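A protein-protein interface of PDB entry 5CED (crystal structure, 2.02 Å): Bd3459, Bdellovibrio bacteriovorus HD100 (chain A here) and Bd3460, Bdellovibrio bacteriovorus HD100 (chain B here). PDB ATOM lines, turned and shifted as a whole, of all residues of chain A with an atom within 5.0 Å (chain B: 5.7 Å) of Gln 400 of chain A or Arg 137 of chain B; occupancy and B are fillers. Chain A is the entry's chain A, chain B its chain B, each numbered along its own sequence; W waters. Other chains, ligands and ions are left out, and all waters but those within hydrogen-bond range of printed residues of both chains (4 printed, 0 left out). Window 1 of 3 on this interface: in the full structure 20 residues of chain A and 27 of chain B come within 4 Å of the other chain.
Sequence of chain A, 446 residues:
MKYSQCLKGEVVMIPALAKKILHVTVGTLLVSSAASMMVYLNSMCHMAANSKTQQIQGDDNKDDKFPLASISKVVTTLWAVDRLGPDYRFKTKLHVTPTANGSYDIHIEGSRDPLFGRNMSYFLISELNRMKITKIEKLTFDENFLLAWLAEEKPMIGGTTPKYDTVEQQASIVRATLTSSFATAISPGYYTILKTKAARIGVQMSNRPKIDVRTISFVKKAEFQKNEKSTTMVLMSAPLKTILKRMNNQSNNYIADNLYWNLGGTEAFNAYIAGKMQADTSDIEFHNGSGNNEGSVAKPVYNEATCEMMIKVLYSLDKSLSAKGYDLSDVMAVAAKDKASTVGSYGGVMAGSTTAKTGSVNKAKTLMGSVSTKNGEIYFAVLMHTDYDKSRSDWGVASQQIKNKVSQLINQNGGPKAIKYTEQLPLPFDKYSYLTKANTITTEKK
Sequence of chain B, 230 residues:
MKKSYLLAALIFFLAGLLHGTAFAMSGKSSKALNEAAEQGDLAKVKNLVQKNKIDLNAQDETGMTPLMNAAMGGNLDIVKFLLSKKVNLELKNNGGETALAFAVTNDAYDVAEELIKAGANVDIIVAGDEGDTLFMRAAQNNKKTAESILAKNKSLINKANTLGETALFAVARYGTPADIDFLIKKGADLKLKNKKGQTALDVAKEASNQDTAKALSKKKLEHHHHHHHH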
ATOM      1  N   GLY A 396      -2.082   0.532   4.443  1.00  0.00           N
ATOM      2  CA  GLY A 396      -2.955   1.410   5.205  1.00  0.00           C
ATOM      3  C   GLY A 396      -2.892   2.863   4.742  1.00  0.00           C
ATOM      4  O   GLY A 396      -3.923   3.563   4.732  1.00  0.00           O
ATOM      5  N   VAL A 397      -1.687   3.337   4.391  1.00  0.00           N
ATOM      6  CA  VAL A 397      -1.533   4.735   3.963  1.00  0.00           C
ATOM      7  C   VAL A 397      -2.347   4.899   2.661  1.00  0.00           C
ATOM      8  O   VAL A 397      -3.144   5.842   2.503  1.00  0.00           O
ATOM      9  CB  VAL A 397      -0.054   5.104   3.799  1.00  0.00           C
ATOM     10  CG1 VAL A 397       0.134   6.447   3.103  1.00  0.00           C
ATOM     11  CG2 VAL A 397       0.692   5.095   5.144  1.00  0.00           C
ATOM     12  N   ALA A 398      -2.169   3.954   1.735  1.00  0.00           N
ATOM     13  CA  ALA A 398      -2.829   4.035   0.417  1.00  0.00           C
ATOM     14  C   ALA A 398      -4.351   3.933   0.555  1.00  0.00           C
ATOM     15  O   ALA A 398      -5.107   4.604  -0.182  1.00  0.00           O
ATOM     16  CB  ALA A 398      -2.290   2.964  -0.499  1.00  0.00           C
ATOM     17  N   SER A 399      -4.788   3.091   1.491  1.00  0.00           N
ATOM     18  CA  SER A 399      -6.214   2.845   1.680  1.00  0.00           C
ATOM     19  C   SER A 399      -6.918   4.142   2.066  1.00  0.00           C
ATOM     20  O   SER A 399      -7.991   4.483   1.478  1.00  0.00           O
ATOM     21  CB  SER A 399      -6.464   1.753   2.729  1.00  0.00           C
ATOM     22  OG  SER A 399      -7.882   1.564   2.895  1.00  0.00           O
ATOM     23  N   GLN A 400      -6.346   4.901   3.005  1.00  0.00           N
ATOM     24  CA  GLN A 400      -6.996   6.170   3.360  1.00  0.00           C
ATOM     25  C   GLN A 400      -6.941   7.202   2.253  1.00  0.00           C
ATOM     26  O   GLN A 400      -7.882   7.987   2.127  1.00  0.00           O
ATOM     27  CB  GLN A 400      -6.532   6.800   4.731  1.00  0.00           C
ATOM     28  CG  GLN A 400      -7.491   7.861   5.320  1.00  0.00           C
ATOM     29  CD  GLN A 400      -8.911   7.391   5.566  1.00  0.00           C
ATOM     30  OE1 GLN A 400      -9.142   6.397   6.257  1.00  0.00           O
ATOM     31  NE2 GLN A 400      -9.909   8.145   5.025  1.00  0.00           N
ATOM     32  N   GLN A 401      -5.866   7.240   1.488  1.00  0.00           N
ATOM     33  CA  GLN A 401      -5.797   8.187   0.381  1.00  0.00           C
ATOM     34  C   GLN A 401      -6.838   7.858  -0.687  1.00  0.00           C
ATOM     35  O   GLN A 401      -7.400   8.742  -1.281  1.00  0.00           O
ATOM     36  CB  GLN A 401      -4.421   8.214  -0.261  1.00  0.00           C
ATOM     37  CG  GLN A 401      -3.357   8.849   0.656  1.00  0.00           C
ATOM     38  CD  GLN A 401      -2.004   8.928  -0.003  1.00  0.00           C
ATOM     39  OE1 GLN A 401      -1.899   8.846  -1.243  1.00  0.00           O
ATOM     40  NE2 GLN A 401      -0.969   9.180   0.799  1.00  0.00           N
ATOM     41  N   ILE A 402      -7.067   6.586  -0.944  1.00  0.00           N
ATOM     42  CA  ILE A 402      -8.118   6.170  -1.858  1.00  0.00           C
ATOM     43  C   ILE A 402      -9.465   6.603  -1.348  1.00  0.00           C
ATOM     44  O   ILE A 402     -10.263   7.142  -2.115  1.00  0.00           O
ATOM     45  CB  ILE A 402      -8.118   4.661  -2.067  1.00  0.00           C
ATOM     46  CG1 ILE A 402      -6.898   4.228  -2.865  1.00  0.00           C
ATOM     47  CG2 ILE A 402      -9.371   4.181  -2.782  1.00  0.00           C
ATOM     48  CD1 ILE A 402      -6.793   2.690  -2.902  1.00  0.00           C
ATOM     49  N   LYS A 403      -9.715   6.361  -0.065  1.00  0.00           N
ATOM     50  CA  LYS A 403     -10.977   6.778   0.534  1.00  0.00           C
ATOM     51  C   LYS A 403     -11.230   8.272   0.355  1.00  0.00           C
ATOM     52  O   LYS A 403     -12.323   8.689  -0.022  1.00  0.00           O
ATOM     53  CB  LYS A 403     -11.077   6.392   2.000  1.00  0.00           C
ATOM     54  CG  LYS A 403     -11.189   4.890   2.229  1.00  0.00           C
ATOM     55  CD  LYS A 403     -11.031   4.583   3.723  1.00  0.00           C
ATOM     56  CE  LYS A 403     -11.171   3.082   3.962  1.00  0.00           C
ATOM     57  NZ  LYS A 403     -10.930   2.590   5.353  1.00  0.00           N
ATOM     58  N   ASN A 404     -10.220   9.068   0.636  1.00  0.00           N
ATOM     59  CA  ASN A 404     -10.357  10.488   0.527  1.00  0.00           C
ATOM     60  C   ASN A 404     -10.632  10.971  -0.915  1.00  0.00           C
ATOM     61  O   ASN A 404     -11.398  11.906  -1.139  1.00  0.00           O
ATOM     62  CB  ASN A 404      -9.083  11.121   1.103  1.00  0.00           C
ATOM     63  CG  ASN A 404      -9.014  11.008   2.617  1.00  0.00           C
ATOM     64  OD1 ASN A 404      -9.916  10.508   3.312  1.00  0.00           O
ATOM     65  ND2 ASN A 404      -7.985  11.519   3.132  1.00  0.00           N
ATOM     66  N   VAL B 104      -6.207  -1.097  12.770  1.00  0.00           N
ATOM     67  CA  VAL B 104      -7.094   0.025  12.436  1.00  0.00           C
ATOM     68  C   VAL B 104      -6.948   0.442  10.957  1.00  0.00           C
ATOM     69  O   VAL B 104      -7.985   0.589  10.236  1.00  0.00           O
ATOM     70  CB  VAL B 104      -6.902   1.180  13.421  1.00  0.00           C
ATOM     71  CG1 VAL B 104      -7.478   2.506  12.947  1.00  0.00           C
ATOM     72  CG2 VAL B 104      -7.501   0.815  14.776  1.00  0.00           C
ATOM     73  N   THR B 105      -5.701   0.636  10.521  1.00  0.00           N
ATOM     74  CA  THR B 105      -5.408   1.145   9.197  1.00  0.00           C
ATOM     75  C   THR B 105      -5.758   0.163   8.064  1.00  0.00           C
ATOM     76  O   THR B 105      -5.952   0.606   6.930  1.00  0.00           O
ATOM     77  CB  THR B 105      -3.930   1.583   9.029  1.00  0.00           C
ATOM     78  OG1 THR B 105      -3.077   0.458   9.246  1.00  0.00           O
ATOM     79  CG2 THR B 105      -3.558   2.779   9.983  1.00  0.00           C
ATOM     80  N   TYR B 109     -11.188  -4.263  12.355  1.00  0.00           N
ATOM     81  CA  TYR B 109     -11.688  -3.607  13.558  1.00  0.00           C
ATOM     82  C   TYR B 109     -12.046  -4.613  14.650  1.00  0.00           C
ATOM     83  O   TYR B 109     -11.987  -4.265  15.813  1.00  0.00           O
ATOM     84  CB  TYR B 109     -12.851  -2.637  13.263  1.00  0.00           C
ATOM     85  CG  TYR B 109     -12.304  -1.327  12.702  1.00  0.00           C
ATOM     86  CD1 TYR B 109     -11.683  -0.406  13.543  1.00  0.00           C
ATOM     87  CD2 TYR B 109     -12.357  -1.030  11.308  1.00  0.00           C
ATOM     88  CE1 TYR B 109     -11.142   0.784  13.070  1.00  0.00           C
ATOM     89  CE2 TYR B 109     -11.807   0.179  10.810  1.00  0.00           C
ATOM     90  CZ  TYR B 109     -11.199   1.075  11.702  1.00  0.00           C
ATOM     91  OH  TYR B 109     -10.672   2.268  11.277  1.00  0.00           O
ATOM     92  N   VAL B 126      -0.521   6.720  13.346  1.00  0.00           N
ATOM     93  CA  VAL B 126      -0.477   5.791  12.179  1.00  0.00           C
ATOM     94  C   VAL B 126       0.404   6.383  11.103  1.00  0.00           C
ATOM     95  O   VAL B 126       0.714   7.575  11.135  1.00  0.00           O
ATOM     96  CB  VAL B 126      -1.919   5.524  11.621  1.00  0.00           C
ATOM     97  CG1 VAL B 126      -2.819   4.988  12.720  1.00  0.00           C
ATOM     98  CG2 VAL B 126      -2.547   6.769  10.995  1.00  0.00           C
ATOM     99  N   ALA B 127       0.828   5.563  10.139  1.00  0.00           N
ATOM    100  CA  ALA B 127       1.841   5.999   9.145  1.00  0.00           C
ATOM    101  C   ALA B 127       1.248   7.022   8.164  1.00  0.00           C
ATOM    102  O   ALA B 127       0.037   7.111   8.038  1.00  0.00           O
ATOM    103  CB  ALA B 127       2.383   4.804   8.387  1.00  0.00           C
ATOM    104  N   GLU B 130       0.809  13.058   7.356  1.00  0.00           N
ATOM    105  CA  GLU B 130      -0.063  13.829   8.285  1.00  0.00           C
ATOM    106  C   GLU B 130       0.182  13.539   9.789  1.00  0.00           C
ATOM    107  O   GLU B 130      -0.101  14.404  10.641  1.00  0.00           O
ATOM    108  CB  GLU B 130      -1.557  13.588   8.012  1.00  0.00           C
ATOM    109  CG  GLU B 130      -1.968  13.601   6.546  1.00  0.00           C
ATOM    110  CD  GLU B 130      -1.827  12.234   5.864  1.00  0.00           C
ATOM    111  OE1 GLU B 130      -1.399  11.234   6.506  1.00  0.00           O
ATOM    112  OE2 GLU B 130      -2.123  12.193   4.659  1.00  0.00           O
ATOM    113  N   ASP B 132      -1.594  11.230  11.471  1.00  0.00           N
ATOM    114  CA  ASP B 132      -2.915  11.097  12.012  1.00  0.00           C
ATOM    115  C   ASP B 132      -2.821  10.238  13.289  1.00  0.00           C
ATOM    116  O   ASP B 132      -1.998   9.303  13.371  1.00  0.00           O
ATOM    117  CB  ASP B 132      -3.883  10.419  11.037  1.00  0.00           C
ATOM    118  CG  ASP B 132      -4.386  11.316   9.977  1.00  0.00           C
ATOM    119  OD1 ASP B 132      -4.170  12.571  10.032  1.00  0.00           O
ATOM    120  OD2 ASP B 132      -4.994  10.752   9.021  1.00  0.00           O
ATOM    121  N   THR B 133      -3.702  10.548  14.239  1.00  0.00           N
ATOM    122  CA  THR B 133      -3.801   9.747  15.432  1.00  0.00           C
ATOM    123  C   THR B 133      -4.626   8.510  15.082  1.00  0.00           C
ATOM    124  O   THR B 133      -5.389   8.495  14.133  1.00  0.00           O
ATOM    125  CB  THR B 133      -4.479  10.470  16.600  1.00  0.00           C
ATOM    126  OG1 THR B 133      -5.834  10.808  16.234  1.00  0.00           O
ATOM    127  CG2 THR B 133      -3.699  11.726  16.954  1.00  0.00           C
ATOM    128  N   LEU B 134      -4.433   7.479  15.867  1.00  0.00           N
ATOM    129  CA  LEU B 134      -5.255   6.309  15.770  1.00  0.00           C
ATOM    130  C   LEU B 134      -6.702   6.655  15.898  1.00  0.00           C
ATOM    131  O   LEU B 134      -7.504   6.146  15.120  1.00  0.00           O
ATOM    132  CB  LEU B 134      -4.890   5.313  16.838  1.00  0.00           C
ATOM    133  CG  LEU B 134      -5.520   3.941  16.694  1.00  0.00           C
ATOM    134  CD1 LEU B 134      -4.719   3.179  15.611  1.00  0.00           C
ATOM    135  CD2 LEU B 134      -5.477   3.230  18.052  1.00  0.00           C
ATOM    136  N   PHE B 135      -7.040   7.518  16.866  1.00  0.00           N
ATOM    137  CA  PHE B 135      -8.403   7.968  17.022  1.00  0.00           C
ATOM    138  C   PHE B 135      -8.987   8.539  15.715  1.00  0.00           C
ATOM    139  O   PHE B 135     -10.156   8.231  15.340  1.00  0.00           O
ATOM    140  CB  PHE B 135      -8.600   8.983  18.166  1.00  0.00           C
ATOM    141  CG  PHE B 135     -10.003   9.458  18.242  1.00  0.00           C
ATOM    142  CD1 PHE B 135     -11.013   8.586  18.594  1.00  0.00           C
ATOM    143  CD2 PHE B 135     -10.349  10.710  17.780  1.00  0.00           C
ATOM    144  CE1 PHE B 135     -12.342   8.992  18.586  1.00  0.00           C
ATOM    145  CE2 PHE B 135     -11.670  11.134  17.774  1.00  0.00           C
ATOM    146  CZ  PHE B 135     -12.673  10.276  18.156  1.00  0.00           C
ATOM    147  N   MET B 136      -8.205   9.392  15.049  1.00  0.00           N
ATOM    148  CA  MET B 136      -8.680  10.080  13.843  1.00  0.00           C
ATOM    149  C   MET B 136      -8.938   9.071  12.758  1.00  0.00           C
ATOM    150  O   MET B 136      -9.931   9.191  12.015  1.00  0.00           O
ATOM    151  CB  MET B 136      -7.668  11.097  13.308  1.00  0.00           C
ATOM    152  CG  MET B 136      -7.595  12.349  14.124  1.00  0.00           C
ATOM    153  SD  MET B 136      -6.139  13.304  13.634  1.00  0.00           S
ATOM    154  CE  MET B 136      -6.692  13.846  12.022  1.00  0.00           C
ATOM    155  N   ARG B 137      -8.083   8.064  12.659  1.00  0.00           N
ATOM    156  CA  ARG B 137      -8.335   7.053  11.615  1.00  0.00           C
ATOM    157  C   ARG B 137      -9.571   6.218  11.898  1.00  0.00           C
ATOM    158  O   ARG B 137     -10.380   5.971  10.987  1.00  0.00           O
ATOM    159  CB  ARG B 137      -7.109   6.175  11.372  1.00  0.00           C
ATOM    160  CG  ARG B 137      -7.199   5.179  10.202  1.00  0.00           C
ATOM    161  CD  ARG B 137      -7.417   5.839   8.852  1.00  0.00           C
ATOM    162  NE  ARG B 137      -6.496   6.953   8.643  1.00  0.00           N
ATOM    163  CZ  ARG B 137      -5.236   6.867   8.169  1.00  0.00           C
ATOM    164  NH1 ARG B 137      -4.712   5.717   7.747  1.00  0.00           N
ATOM    165  NH2 ARG B 137      -4.512   7.976   8.054  1.00  0.00           N
ATOM    166  N   ALA B 138      -9.739   5.802  13.151  1.00  0.00           N
ATOM    167  CA  ALA B 138     -10.922   5.033  13.543  1.00  0.00           C
ATOM    168  C   ALA B 138     -12.198   5.869  13.368  1.00  0.00           C
ATOM    169  O   ALA B 138     -13.230   5.364  12.891  1.00  0.00           O
ATOM    170  CB  ALA B 138     -10.803   4.514  14.963  1.00  0.00           C
ATOM    171  N   ALA B 139     -12.123   7.134  13.745  1.00  0.00           N
ATOM    172  CA  ALA B 139     -13.263   8.028  13.666  1.00  0.00           C
ATOM    173  C   ALA B 139     -13.810   8.216  12.264  1.00  0.00           C
ATOM    174  O   ALA B 139     -15.003   8.437  12.101  1.00  0.00           O
ATOM    175  CB  ALA B 139     -12.922   9.403  14.274  1.00  0.00           C
ATOM    176  N   GLN B 140     -12.948   8.166  11.253  1.00  0.00           N
ATOM    177  CA  GLN B 140     -13.445   8.241   9.886  1.00  0.00           C
ATOM    178  C   GLN B 140     -14.147   6.955   9.416  1.00  0.00           C
ATOM    179  O   GLN B 140     -14.823   6.988   8.397  1.00  0.00           O
ATOM    180  CB  GLN B 140     -12.290   8.568   8.924  1.00  0.00           C
ATOM    181  CG  GLN B 140     -11.850  10.030   8.941  1.00  0.00           C
ATOM    182  CD  GLN B 140     -10.940  10.344   7.755  1.00  0.00           C
ATOM    183  OE1 GLN B 140      -9.744  10.241   7.860  1.00  0.00           O
ATOM    184  NE2 GLN B 140     -11.515  10.634   6.628  1.00  0.00           N
ATOM    185  N   ASN B 141     -13.972   5.833  10.117  1.00  0.00           N
ATOM    186  CA  ASN B 141     -14.376   4.517   9.607  1.00  0.00           C
ATOM    187  C   ASN B 141     -15.273   3.706  10.542  1.00  0.00           C
ATOM    188  O   ASN B 141     -16.359   3.330  10.147  1.00  0.00           O
ATOM    189  CB  ASN B 141     -13.130   3.729   9.209  1.00  0.00           C
ATOM    190  CG  ASN B 141     -12.403   4.357   8.031  1.00  0.00           C
ATOM    191  OD1 ASN B 141     -12.852   4.236   6.890  1.00  0.00           O
ATOM    192  ND2 ASN B 141     -11.354   5.081   8.300  1.00  0.00           N
ATOM    193  N   ASN B 142     -14.831   3.450  11.760  1.00  0.00           N
ATOM    194  CA  ASN B 142     -15.516   2.520  12.657  1.00  0.00           C
ATOM    195  C   ASN B 142     -15.806   3.209  14.000  1.00  0.00           C
ATOM    196  O   ASN B 142     -14.920   3.413  14.835  1.00  0.00           O
ATOM    197  CB  ASN B 142     -14.708   1.236  12.858  1.00  0.00           C
ATOM    198  CG  ASN B 142     -15.482   0.176  13.637  1.00  0.00           C
ATOM    199  OD1 ASN B 142     -15.547   0.226  14.864  1.00  0.00           O
ATOM    200  ND2 ASN B 142     -16.056  -0.791  12.937  1.00  0.00           N
HETATM  201  O   HOH W   1      -8.125   0.332   5.070  1.00  0.00           O
HETATM  202  O   HOH W   2      -1.160   9.976   3.557  1.00  0.00           O
HETATM  203  O   HOH W   3      -5.945   3.312   6.576  1.00  0.00           O
HETATM  204  O   HOH W   4      -8.375  11.943   6.090  1.00  0.00           O
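Of the 17 printed residues of chain B, 5 touch a printed residue of chain A. Printed residues of chain B that touch a printed residue of chain A: Thr 105, Ala 127, Arg 137, Gln 140 and Asn 141. Hydrophobic or aromatic side chains of chain B that line the printed part of chain A: Ala 127.
The side-chain amide oxygen of Gln 400 of chain A sits at hydrogen-bond distance from the side-chain amide nitrogen of Asn 141 of chain B, at 3.3 Å. The side-chain amide nitrogen (NE2) of Gln 400 of chain A lies close to the side-chain amide nitrogen (NE2) of Gln 140 of chain B (3.4 Å). The side-chain amino group of Lys 403 of chain A lies within hydrogen-bond range of the side-chain amide oxygen of Asn 141 of chain B (3.0 Å).
The side-chain amide nitrogen of Gln 400 of chain A is in hydrogen-bond range of the side-chain amide oxygen of Asn 404 of chain A (2.9 Å). The guanidinium group (NH2) of Arg 137 of chain B lies within salt-bridge range of the side-chain carboxylate (OD2) of Asp 132 of chain B, 3.0 Å away. The side-chain amide nitrogen (ND2) of Asn 141 of chain B is in hydrogen-bond range of the backbone carbonyl oxygen (O) of Arg 137 of chain B, at 3.0 Å.
Ala 398 of chain A touches none of the printed residues of chain B. Gln 400 of chain A touches just these residues of chain B: Arg 137 (3.2 Å), Gln 140 (3.4 Å) and Asn 141 (3.3 Å). Printed residues of chain A within 4 Å of Ala 127 of chain B: Val 397. Of chain A, only Gly 396 (3.8 Å) and Gln 400 (3.2 Å) come within 4 Å of Arg 137 of chain B. Printed residues of chain A within 4 Å of Gln 140 of chain B: Gln 400 and Asn 404. The nearest residue of chain B that does not touch Gln 400 of chain A is Asp 132 of chain B (5.3 Å). The nearest printed residue of chain A that does not touch Arg 137 of chain B is Val 397 of chain A (5.0 Å).
O of Thr 105 of chain B touches CA of Gly 396 of chain A, at 3.6 Å. NH1 of Arg 137 of chain B touches O of Gly 396 of chain A, at 3.8 Å. CG2 of Val 397 of chain A touches O of Ala 127 of chain B (3.6 Å). Arg 137 of chain B touches Gln 400 of chain A (CD to OE1, 3.2 Å). Asn 404 of chain A touches Gln 140 of chain B (OD1 to NE2, 3.7 Å).
Water W1 lies within hydrogen-bond range of OG of Ser 399 of chain A (2.5 Å) and O of Thr 105 of chain B (2.9 Å). Water W2 bridges OE2 of Glu 130 of chain B (2.7 Å) and NE2 of Gln 401 of chain A (2.9 Å). Water W3 lies within hydrogen-bond range of the backbone carbonyl oxygen of Thr 105 of chain B, the backbone carbonyl oxygen of Gly 396 of chain A and the guanidinium group of Arg 137 of chain B. Water W4 bridges OE1 of Gln 140 of chain B (2.8 Å) and ND2 of Asn 404 of chain A (3.0 Å).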
